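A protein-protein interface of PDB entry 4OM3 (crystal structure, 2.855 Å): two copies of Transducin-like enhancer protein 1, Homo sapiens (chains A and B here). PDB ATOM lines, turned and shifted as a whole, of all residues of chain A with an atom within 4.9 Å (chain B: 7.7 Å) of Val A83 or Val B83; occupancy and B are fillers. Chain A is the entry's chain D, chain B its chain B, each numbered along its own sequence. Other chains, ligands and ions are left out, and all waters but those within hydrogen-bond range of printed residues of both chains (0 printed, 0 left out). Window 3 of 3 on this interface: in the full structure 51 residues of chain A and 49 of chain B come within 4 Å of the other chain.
Printed residues of chain A that touch a printed residue of chain B: Ile A79, Cys A80, Val A83, Phe A86, Leu A87 and Val A95. Hydrophobic or aromatic side chains of chain A within 4 Å of the printed part of chain B: Ile A79, Val A83, Phe A86, Leu A87 and Val A95. Of the 19 printed residues of chain B, 6 touch a printed residue of chain A. Printed residues of chain B that touch a printed residue of chain A: Cys B80, Val B83, His B91, Val B95, Ala B98 and Val B99.
The side-chain sulfur of Cys A80 is in hydrogen-bond range of the side-chain sulfur of Cys B80 (3.4 Å).
Val A83 touches just these residues of chain B: Val B83 and Val B95. Val B83 touches three residues of chain A. Printed residues of chain B within 4 Å of Phe A86: His B91. Of the printed residues of chain A, Ala B98 touches Ile A79 (3.4 Å). Of the printed residues of chain A, Cys B80 touches Cys A80. Of the printed residues of chain B, Leu A87 touches Val B83 (3.7 Å). Of the printed residues of chain A, His B91 touches Phe A86 (3.3 Å). The nearest residue of chain B that does not touch Val A83 is Leu B87 (4.03 Å). The nearest printed residue of chain A that does not touch Val B83 is Ile A84 (5.8 Å).
The backbone carbonyl oxygen (O) of Leu B76 lies within hydrogen-bond range of the side-chain sulfur (SG) of Cys B80, 3.4 Å away.
Cys B80 touches its own counterpart, Cys A80. Val A83 touches its own counterpart, Val B83. Val A83 touches Val B95, and with the chains exchanged Val A95 touches Val B83. Leu A87 touches Val B83, but with the chains exchanged Val A83 does not touch Leu B87 (4.03 Å). Positions printed for both chains: 79, 80, 81, 82, 83, 84, 85, 86, 87 and 95.
Ile A79 touches Val B95 (CG2 to CG1, 3.97 Å). Ile A79 touches Ala B98. Ile A79 touches Val B99. Val A83 touches Val B83. CG2 of Val B95 touches CG2 of Val A83 (3.6 Å). CD2 of Phe A86 touches NE2 of His B91, at 3.3 Å. CD1 of Leu A87 touches CG1 of Val B83, at 3.7 Å. Val A95 touches Val B83 (CG2 to CG2, 3.6 Å).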
ATOM      1  N   ILE A  79      18.459 -31.829   5.141  1.00  0.00           N
ATOM      2  CA  ILE A  79      19.576 -31.536   4.244  1.00  0.00           C
ATOM      3  C   ILE A  79      20.745 -30.883   4.982  1.00  0.00           C
ATOM      4  O   ILE A  79      21.906 -31.242   4.762  1.00  0.00           O
ATOM      5  CB  ILE A  79      19.140 -30.652   3.061  1.00  0.00           C
ATOM      6  CG1 ILE A  79      18.007 -31.330   2.289  1.00  0.00           C
ATOM      7  CG2 ILE A  79      20.315 -30.373   2.136  1.00  0.00           C
ATOM      8  CD1 ILE A  79      17.539 -30.554   1.087  1.00  0.00           C
ATOM      9  N   CYS A  80      20.438 -29.931   5.860  1.00  0.00           N
ATOM     10  CA  CYS A  80      21.464 -29.323   6.704  1.00  0.00           C
ATOM     11  C   CYS A  80      22.114 -30.380   7.586  1.00  0.00           C
ATOM     12  O   CYS A  80      23.340 -30.429   7.717  1.00  0.00           O
ATOM     13  CB  CYS A  80      20.869 -28.221   7.581  1.00  0.00           C
ATOM     14  SG  CYS A  80      20.478 -26.687   6.721  1.00  0.00           S
ATOM     15  N   ALA A  81      21.279 -31.229   8.180  1.00  0.00           N
ATOM     16  CA  ALA A  81      21.747 -32.288   9.066  1.00  0.00           C
ATOM     17  C   ALA A  81      22.748 -33.202   8.370  1.00  0.00           C
ATOM     18  O   ALA A  81      23.720 -33.651   8.977  1.00  0.00           O
ATOM     19  CB  ALA A  81      20.568 -33.094   9.590  1.00  0.00           C
ATOM     20  N   GLN A  82      22.509 -33.465   7.089  1.00  0.00           N
ATOM     21  CA  GLN A  82      23.380 -34.340   6.315  1.00  0.00           C
ATOM     22  C   GLN A  82      24.627 -33.618   5.816  1.00  0.00           C
ATOM     23  O   GLN A  82      25.692 -34.223   5.685  1.00  0.00           O
ATOM     24  CB  GLN A  82      22.616 -34.930   5.130  1.00  0.00           C
ATOM     25  CG  GLN A  82      21.419 -35.776   5.523  1.00  0.00           C
ATOM     26  CD  GLN A  82      20.519 -36.083   4.347  1.00  0.00           C
ATOM     27  OE1 GLN A  82      20.465 -35.324   3.378  1.00  0.00           O
ATOM     28  NE2 GLN A  82      19.805 -37.201   4.421  1.00  0.00           N
ATOM     29  N   VAL A  83      24.496 -32.324   5.537  1.00  0.00           N
ATOM     30  CA  VAL A  83      25.594 -31.569   4.941  1.00  0.00           C
ATOM     31  C   VAL A  83      26.602 -31.064   5.978  1.00  0.00           C
ATOM     32  O   VAL A  83      27.751 -30.778   5.642  1.00  0.00           O
ATOM     33  CB  VAL A  83      25.078 -30.391   4.078  1.00  0.00           C
ATOM     34  CG1 VAL A  83      26.235 -29.544   3.566  1.00  0.00           C
ATOM     35  CG2 VAL A  83      24.247 -30.910   2.918  1.00  0.00           C
ATOM     36  N   ILE A  84      26.170 -30.965   7.232  1.00  0.00           N
ATOM     37  CA  ILE A  84      27.043 -30.501   8.314  1.00  0.00           C
ATOM     38  C   ILE A  84      28.334 -31.317   8.543  1.00  0.00           C
ATOM     39  O   ILE A  84      29.418 -30.734   8.606  1.00  0.00           O
ATOM     40  CB  ILE A  84      26.271 -30.324   9.650  1.00  0.00           C
ATOM     41  CG1 ILE A  84      25.408 -29.064   9.601  1.00  0.00           C
ATOM     42  CG2 ILE A  84      27.233 -30.244  10.825  1.00  0.00           C
ATOM     43  CD1 ILE A  84      24.660 -28.785  10.886  1.00  0.00           C
ATOM     44  N   PRO A  85      28.236 -32.659   8.654  1.00  0.00           N
ATOM     45  CA  PRO A  85      29.445 -33.429   8.989  1.00  0.00           C
ATOM     46  C   PRO A  85      30.578 -33.387   7.954  1.00  0.00           C
ATOM     47  O   PRO A  85      31.582 -34.071   8.144  1.00  0.00           O
ATOM     48  CB  PRO A  85      28.917 -34.864   9.129  1.00  0.00           C
ATOM     49  CG  PRO A  85      27.653 -34.885   8.350  1.00  0.00           C
ATOM     50  CD  PRO A  85      27.054 -33.535   8.555  1.00  0.00           C
ATOM     51  N   PHE A  86      30.426 -32.603   6.892  1.00  0.00           N
ATOM     52  CA  PHE A  86      31.473 -32.466   5.884  1.00  0.00           C
ATOM     53  C   PHE A  86      32.425 -31.315   6.200  1.00  0.00           C
ATOM     54  O   PHE A  86      33.463 -31.166   5.556  1.00  0.00           O
ATOM     55  CB  PHE A  86      30.858 -32.241   4.501  1.00  0.00           C
ATOM     56  CG  PHE A  86      30.391 -33.499   3.825  1.00  0.00           C
ATOM     57  CD1 PHE A  86      29.183 -34.081   4.170  1.00  0.00           C
ATOM     58  CD2 PHE A  86      31.156 -34.090   2.834  1.00  0.00           C
ATOM     59  CE1 PHE A  86      28.750 -35.235   3.543  1.00  0.00           C
ATOM     60  CE2 PHE A  86      30.729 -35.243   2.205  1.00  0.00           C
ATOM     61  CZ  PHE A  86      29.525 -35.816   2.560  1.00  0.00           C
ATOM     62  N   LEU A  87      32.071 -30.508   7.195  1.00  0.00           N
ATOM     63  CA  LEU A  87      32.764 -29.245   7.441  1.00  0.00           C
ATOM     64  C   LEU A  87      33.843 -29.315   8.517  1.00  0.00           C
ATOM     65  O   LEU A  87      33.994 -30.323   9.210  1.00  0.00           O
ATOM     66  CB  LEU A  87      31.753 -28.161   7.814  1.00  0.00           C
ATOM     67  CG  LEU A  87      30.572 -27.964   6.865  1.00  0.00           C
ATOM     68  CD1 LEU A  87      29.557 -27.021   7.484  1.00  0.00           C
ATOM     69  CD2 LEU A  87      31.043 -27.440   5.519  1.00  0.00           C
ATOM     70  N   VAL A  95      27.467 -23.694  12.126  1.00  0.00           N
ATOM     71  CA  VAL A  95      26.277 -23.979  11.332  1.00  0.00           C
ATOM     72  C   VAL A  95      25.182 -24.668  12.149  1.00  0.00           C
ATOM     73  O   VAL A  95      24.017 -24.312  12.027  1.00  0.00           O
ATOM     74  CB  VAL A  95      26.590 -24.767  10.029  1.00  0.00           C
ATOM     75  CG1 VAL A  95      27.275 -26.083  10.332  1.00  0.00           C
ATOM     76  CG2 VAL A  95      25.316 -25.005   9.235  1.00  0.00           C
ATOM     77  N   LEU B  76      16.369 -21.657   6.978  1.00  0.00           N
ATOM     78  CA  LEU B  76      17.106 -22.883   6.674  1.00  0.00           C
ATOM     79  C   LEU B  76      17.622 -22.883   5.241  1.00  0.00           C
ATOM     80  O   LEU B  76      18.774 -23.248   4.985  1.00  0.00           O
ATOM     81  CB  LEU B  76      16.244 -24.122   6.907  1.00  0.00           C
ATOM     82  CG  LEU B  76      15.865 -24.391   8.362  1.00  0.00           C
ATOM     83  CD1 LEU B  76      15.265 -25.784   8.527  1.00  0.00           C
ATOM     84  CD2 LEU B  76      17.081 -24.219   9.244  1.00  0.00           C
ATOM     85  N   ASN B  77      16.769 -22.463   4.313  1.00  0.00           N
ATOM     86  CA  ASN B  77      17.170 -22.315   2.922  1.00  0.00           C
ATOM     87  C   ASN B  77      18.361 -21.371   2.798  1.00  0.00           C
ATOM     88  O   ASN B  77      19.333 -21.665   2.092  1.00  0.00           O
ATOM     89  CB  ASN B  77      15.995 -21.801   2.088  1.00  0.00           C
ATOM     90  CG  ASN B  77      16.343 -21.648   0.625  1.00  0.00           C
ATOM     91  OD1 ASN B  77      16.316 -22.615  -0.137  1.00  0.00           O
ATOM     92  ND2 ASN B  77      16.673 -20.428   0.220  1.00  0.00           N
ATOM     93  N   THR B  78      18.287 -20.245   3.504  1.00  0.00           N
ATOM     94  CA  THR B  78      19.360 -19.257   3.468  1.00  0.00           C
ATOM     95  C   THR B  78      20.690 -19.819   3.980  1.00  0.00           C
ATOM     96  O   THR B  78      21.753 -19.500   3.439  1.00  0.00           O
ATOM     97  CB  THR B  78      18.968 -17.947   4.207  1.00  0.00           C
ATOM     98  OG1 THR B  78      18.653 -18.245   5.573  1.00  0.00           O
ATOM     99  CG2 THR B  78      17.768 -17.270   3.554  1.00  0.00           C
ATOM    100  N   ILE B  79      20.645 -20.673   4.999  1.00  0.00           N
ATOM    101  CA  ILE B  79      21.898 -21.205   5.532  1.00  0.00           C
ATOM    102  C   ILE B  79      22.415 -22.412   4.749  1.00  0.00           C
ATOM    103  O   ILE B  79      23.607 -22.707   4.788  1.00  0.00           O
ATOM    104  CB  ILE B  79      21.843 -21.497   7.051  1.00  0.00           C
ATOM    105  CG1 ILE B  79      20.779 -22.542   7.379  1.00  0.00           C
ATOM    106  CG2 ILE B  79      21.643 -20.212   7.839  1.00  0.00           C
ATOM    107  CD1 ILE B  79      20.844 -23.010   8.813  1.00  0.00           C
ATOM    108  N   CYS B  80      21.524 -23.104   4.042  1.00  0.00           N
ATOM    109  CA  CYS B  80      21.958 -24.089   3.059  1.00  0.00           C
ATOM    110  C   CYS B  80      22.744 -23.337   2.000  1.00  0.00           C
ATOM    111  O   CYS B  80      23.835 -23.756   1.589  1.00  0.00           O
ATOM    112  CB  CYS B  80      20.761 -24.783   2.407  1.00  0.00           C
ATOM    113  SG  CYS B  80      19.948 -26.036   3.417  1.00  0.00           S
ATOM    114  N   ALA B  81      22.179 -22.210   1.574  1.00  0.00           N
ATOM    115  CA  ALA B  81      22.837 -21.330   0.618  1.00  0.00           C
ATOM    116  C   ALA B  81      24.179 -20.838   1.153  1.00  0.00           C
ATOM    117  O   ALA B  81      25.116 -20.619   0.388  1.00  0.00           O
ATOM    118  CB  ALA B  81      21.938 -20.153   0.272  1.00  0.00           C
ATOM    119  N   GLN B  82      24.270 -20.670   2.468  1.00  0.00           N
ATOM    120  CA  GLN B  82      25.523 -20.244   3.085  1.00  0.00           C
ATOM    121  C   GLN B  82      26.584 -21.348   3.101  1.00  0.00           C
ATOM    122  O   GLN B  82      27.746 -21.105   2.775  1.00  0.00           O
ATOM    123  CB  GLN B  82      25.280 -19.720   4.503  1.00  0.00           C
ATOM    124  CG  GLN B  82      24.578 -18.372   4.555  1.00  0.00           C
ATOM    125  CD  GLN B  82      24.502 -17.807   5.960  1.00  0.00           C
ATOM    126  OE1 GLN B  82      24.646 -18.534   6.943  1.00  0.00           O
ATOM    127  NE2 GLN B  82      24.282 -16.502   6.061  1.00  0.00           N
ATOM    128  N   VAL B  83      26.181 -22.558   3.476  1.00  0.00           N
ATOM    129  CA  VAL B  83      27.125 -23.664   3.624  1.00  0.00           C
ATOM    130  C   VAL B  83      27.623 -24.201   2.286  1.00  0.00           C
ATOM    131  O   VAL B  83      28.813 -24.475   2.134  1.00  0.00           O
ATOM    132  CB  VAL B  83      26.521 -24.829   4.436  1.00  0.00           C
ATOM    133  CG1 VAL B  83      27.527 -25.963   4.571  1.00  0.00           C
ATOM    134  CG2 VAL B  83      26.085 -24.348   5.804  1.00  0.00           C
ATOM    135  N   ILE B  84      26.709 -24.341   1.327  1.00  0.00           N
ATOM    136  CA  ILE B  84      27.028 -24.936   0.019  1.00  0.00           C
ATOM    137  C   ILE B  84      28.369 -24.539  -0.639  1.00  0.00           C
ATOM    138  O   ILE B  84      29.138 -25.418  -1.027  1.00  0.00           O
ATOM    139  CB  ILE B  84      25.857 -24.783  -0.993  1.00  0.00           C
ATOM    140  CG1 ILE B  84      24.771 -25.819  -0.703  1.00  0.00           C
ATOM    141  CG2 ILE B  84      26.349 -24.932  -2.428  1.00  0.00           C
ATOM    142  CD1 ILE B  84      23.631 -25.802  -1.693  1.00  0.00           C
ATOM    143  N   PRO B  85      28.666 -23.228  -0.751  1.00  0.00           N
ATOM    144  CA  PRO B  85      29.883 -22.846  -1.482  1.00  0.00           C
ATOM    145  C   PRO B  85      31.211 -23.309  -0.867  1.00  0.00           C
ATOM    146  O   PRO B  85      32.257 -23.038  -1.452  1.00  0.00           O
ATOM    147  CB  PRO B  85      29.819 -21.315  -1.488  1.00  0.00           C
ATOM    148  CG  PRO B  85      28.375 -21.001  -1.330  1.00  0.00           C
ATOM    149  CD  PRO B  85      27.872 -22.042  -0.383  1.00  0.00           C
ATOM    150  N   PHE B  86      31.177 -23.991   0.274  1.00  0.00           N
ATOM    151  CA  PHE B  86      32.405 -24.492   0.887  1.00  0.00           C
ATOM    152  C   PHE B  86      32.589 -25.986   0.646  1.00  0.00           C
ATOM    153  O   PHE B  86      33.384 -26.637   1.322  1.00  0.00           O
ATOM    154  CB  PHE B  86      32.424 -24.208   2.392  1.00  0.00           C
ATOM    155  CG  PHE B  86      32.376 -22.749   2.737  1.00  0.00           C
ATOM    156  CD1 PHE B  86      33.515 -21.965   2.658  1.00  0.00           C
ATOM    157  CD2 PHE B  86      31.192 -22.163   3.148  1.00  0.00           C
ATOM    158  CE1 PHE B  86      33.472 -20.622   2.979  1.00  0.00           C
ATOM    159  CE2 PHE B  86      31.142 -20.821   3.469  1.00  0.00           C
ATOM    160  CZ  PHE B  86      32.283 -20.049   3.385  1.00  0.00           C
ATOM    161  N   LEU B  87      31.850 -26.527  -0.316  1.00  0.00           N
ATOM    162  CA  LEU B  87      31.926 -27.953  -0.610  1.00  0.00           C
ATOM    163  C   LEU B  87      32.699 -28.215  -1.890  1.00  0.00           C
ATOM    164  O   LEU B  87      33.011 -27.290  -2.640  1.00  0.00           O
ATOM    165  CB  LEU B  87      30.526 -28.548  -0.746  1.00  0.00           C
ATOM    166  CG  LEU B  87      29.547 -28.323   0.404  1.00  0.00           C
ATOM    167  CD1 LEU B  87      28.219 -29.000   0.104  1.00  0.00           C
ATOM    168  CD2 LEU B  87      30.131 -28.825   1.716  1.00  0.00           C
ATOM    169  N   HIS B  91      29.677 -32.378  -4.765  1.00  0.00           N
ATOM    170  CA  HIS B  91      28.908 -32.269  -3.534  1.00  0.00           C
ATOM    171  C   HIS B  91      27.982 -31.057  -3.583  1.00  0.00           C
ATOM    172  O   HIS B  91      26.808 -31.150  -3.221  1.00  0.00           O
ATOM    173  CB  HIS B  91      29.840 -32.173  -2.330  1.00  0.00           C
ATOM    174  CG  HIS B  91      29.206 -32.577  -1.044  1.00  0.00           C
ATOM    175  ND1 HIS B  91      27.978 -33.220  -0.990  1.00  0.00           N
ATOM    176  CD2 HIS B  91      29.605 -32.442   0.239  1.00  0.00           C
ATOM    177  CE1 HIS B  91      27.664 -33.455   0.263  1.00  0.00           C
ATOM    178  NE2 HIS B  91      28.635 -32.992   1.038  1.00  0.00           N
ATOM    179  N   GLN B  92      28.518 -29.925  -4.037  1.00  0.00           N
ATOM    180  CA  GLN B  92      27.728 -28.706  -4.196  1.00  0.00           C
ATOM    181  C   GLN B  92      26.531 -28.952  -5.098  1.00  0.00           C
ATOM    182  O   GLN B  92      25.418 -28.537  -4.789  1.00  0.00           O
ATOM    183  CB  GLN B  92      28.574 -27.574  -4.784  1.00  0.00           C
ATOM    184  CG  GLN B  92      29.580 -26.962  -3.829  1.00  0.00           C
ATOM    185  CD  GLN B  92      30.352 -25.816  -4.456  1.00  0.00           C
ATOM    186  OE1 GLN B  92      29.911 -25.216  -5.437  1.00  0.00           O
ATOM    187  NE2 GLN B  92      31.515 -25.511  -3.894  1.00  0.00           N
ATOM    188  N   GLN B  94      25.062 -31.861  -5.818  1.00  0.00           N
ATOM    189  CA  GLN B  94      24.137 -32.773  -5.151  1.00  0.00           C
ATOM    190  C   GLN B  94      23.263 -32.038  -4.140  1.00  0.00           C
ATOM    191  O   GLN B  94      22.039 -32.180  -4.146  1.00  0.00           O
ATOM    192  CB  GLN B  94      24.899 -33.902  -4.449  1.00  0.00           C
ATOM    193  CG  GLN B  94      25.735 -34.772  -5.375  1.00  0.00           C
ATOM    194  CD  GLN B  94      24.899 -35.548  -6.371  1.00  0.00           C
ATOM    195  OE1 GLN B  94      23.718 -35.808  -6.141  1.00  0.00           O
ATOM    196  NE2 GLN B  94      25.510 -35.925  -7.489  1.00  0.00           N
ATOM    197  N   VAL B  95      23.895 -31.248  -3.277  1.00  0.00           N
ATOM    198  CA  VAL B  95      23.167 -30.519  -2.243  1.00  0.00           C
ATOM    199  C   VAL B  95      22.228 -29.475  -2.843  1.00  0.00           C
ATOM    200  O   VAL B  95      21.107 -29.304  -2.373  1.00  0.00           O
ATOM    201  CB  VAL B  95      24.119 -29.844  -1.236  1.00  0.00           C
ATOM    202  CG1 VAL B  95      23.326 -29.139  -0.146  1.00  0.00           C
ATOM    203  CG2 VAL B  95      25.052 -30.873  -0.625  1.00  0.00           C
ATOM    204  N   ALA B  96      22.689 -28.785  -3.881  1.00  0.00           N
ATOM    205  CA  ALA B  96      21.863 -27.797  -4.567  1.00  0.00           C
ATOM    206  C   ALA B  96      20.631 -28.464  -5.167  1.00  0.00           C
ATOM    207  O   ALA B  96      19.517 -27.959  -5.036  1.00  0.00           O
ATOM    208  CB  ALA B  96      22.663 -27.084  -5.645  1.00  0.00           C
ATOM    209  N   ALA B  98      19.301 -31.199  -4.157  1.00  0.00           N
ATOM    210  CA  ALA B  98      18.476 -31.684  -3.054  1.00  0.00           C
ATOM    211  C   ALA B  98      17.631 -30.577  -2.423  1.00  0.00           C
ATOM    212  O   ALA B  98      16.457 -30.785  -2.118  1.00  0.00           O
ATOM    213  CB  ALA B  98      19.340 -32.363  -2.003  1.00  0.00           C
ATOM    214  N   VAL B  99      18.237 -29.411  -2.219  1.00  0.00           N
ATOM    215  CA  VAL B  99      17.530 -28.252  -1.683  1.00  0.00           C
ATOM    216  C   VAL B  99      16.453 -27.825  -2.664  1.00  0.00           C
ATOM    217  O   VAL B  99      15.309 -27.566  -2.284  1.00  0.00           O
ATOM    218  CB  VAL B  99      18.485 -27.067  -1.446  1.00  0.00           C
ATOM    219  CG1 VAL B  99      17.703 -25.804  -1.116  1.00  0.00           C
ATOM    220  CG2 VAL B  99      19.474 -27.394  -0.338  1.00  0.00           C
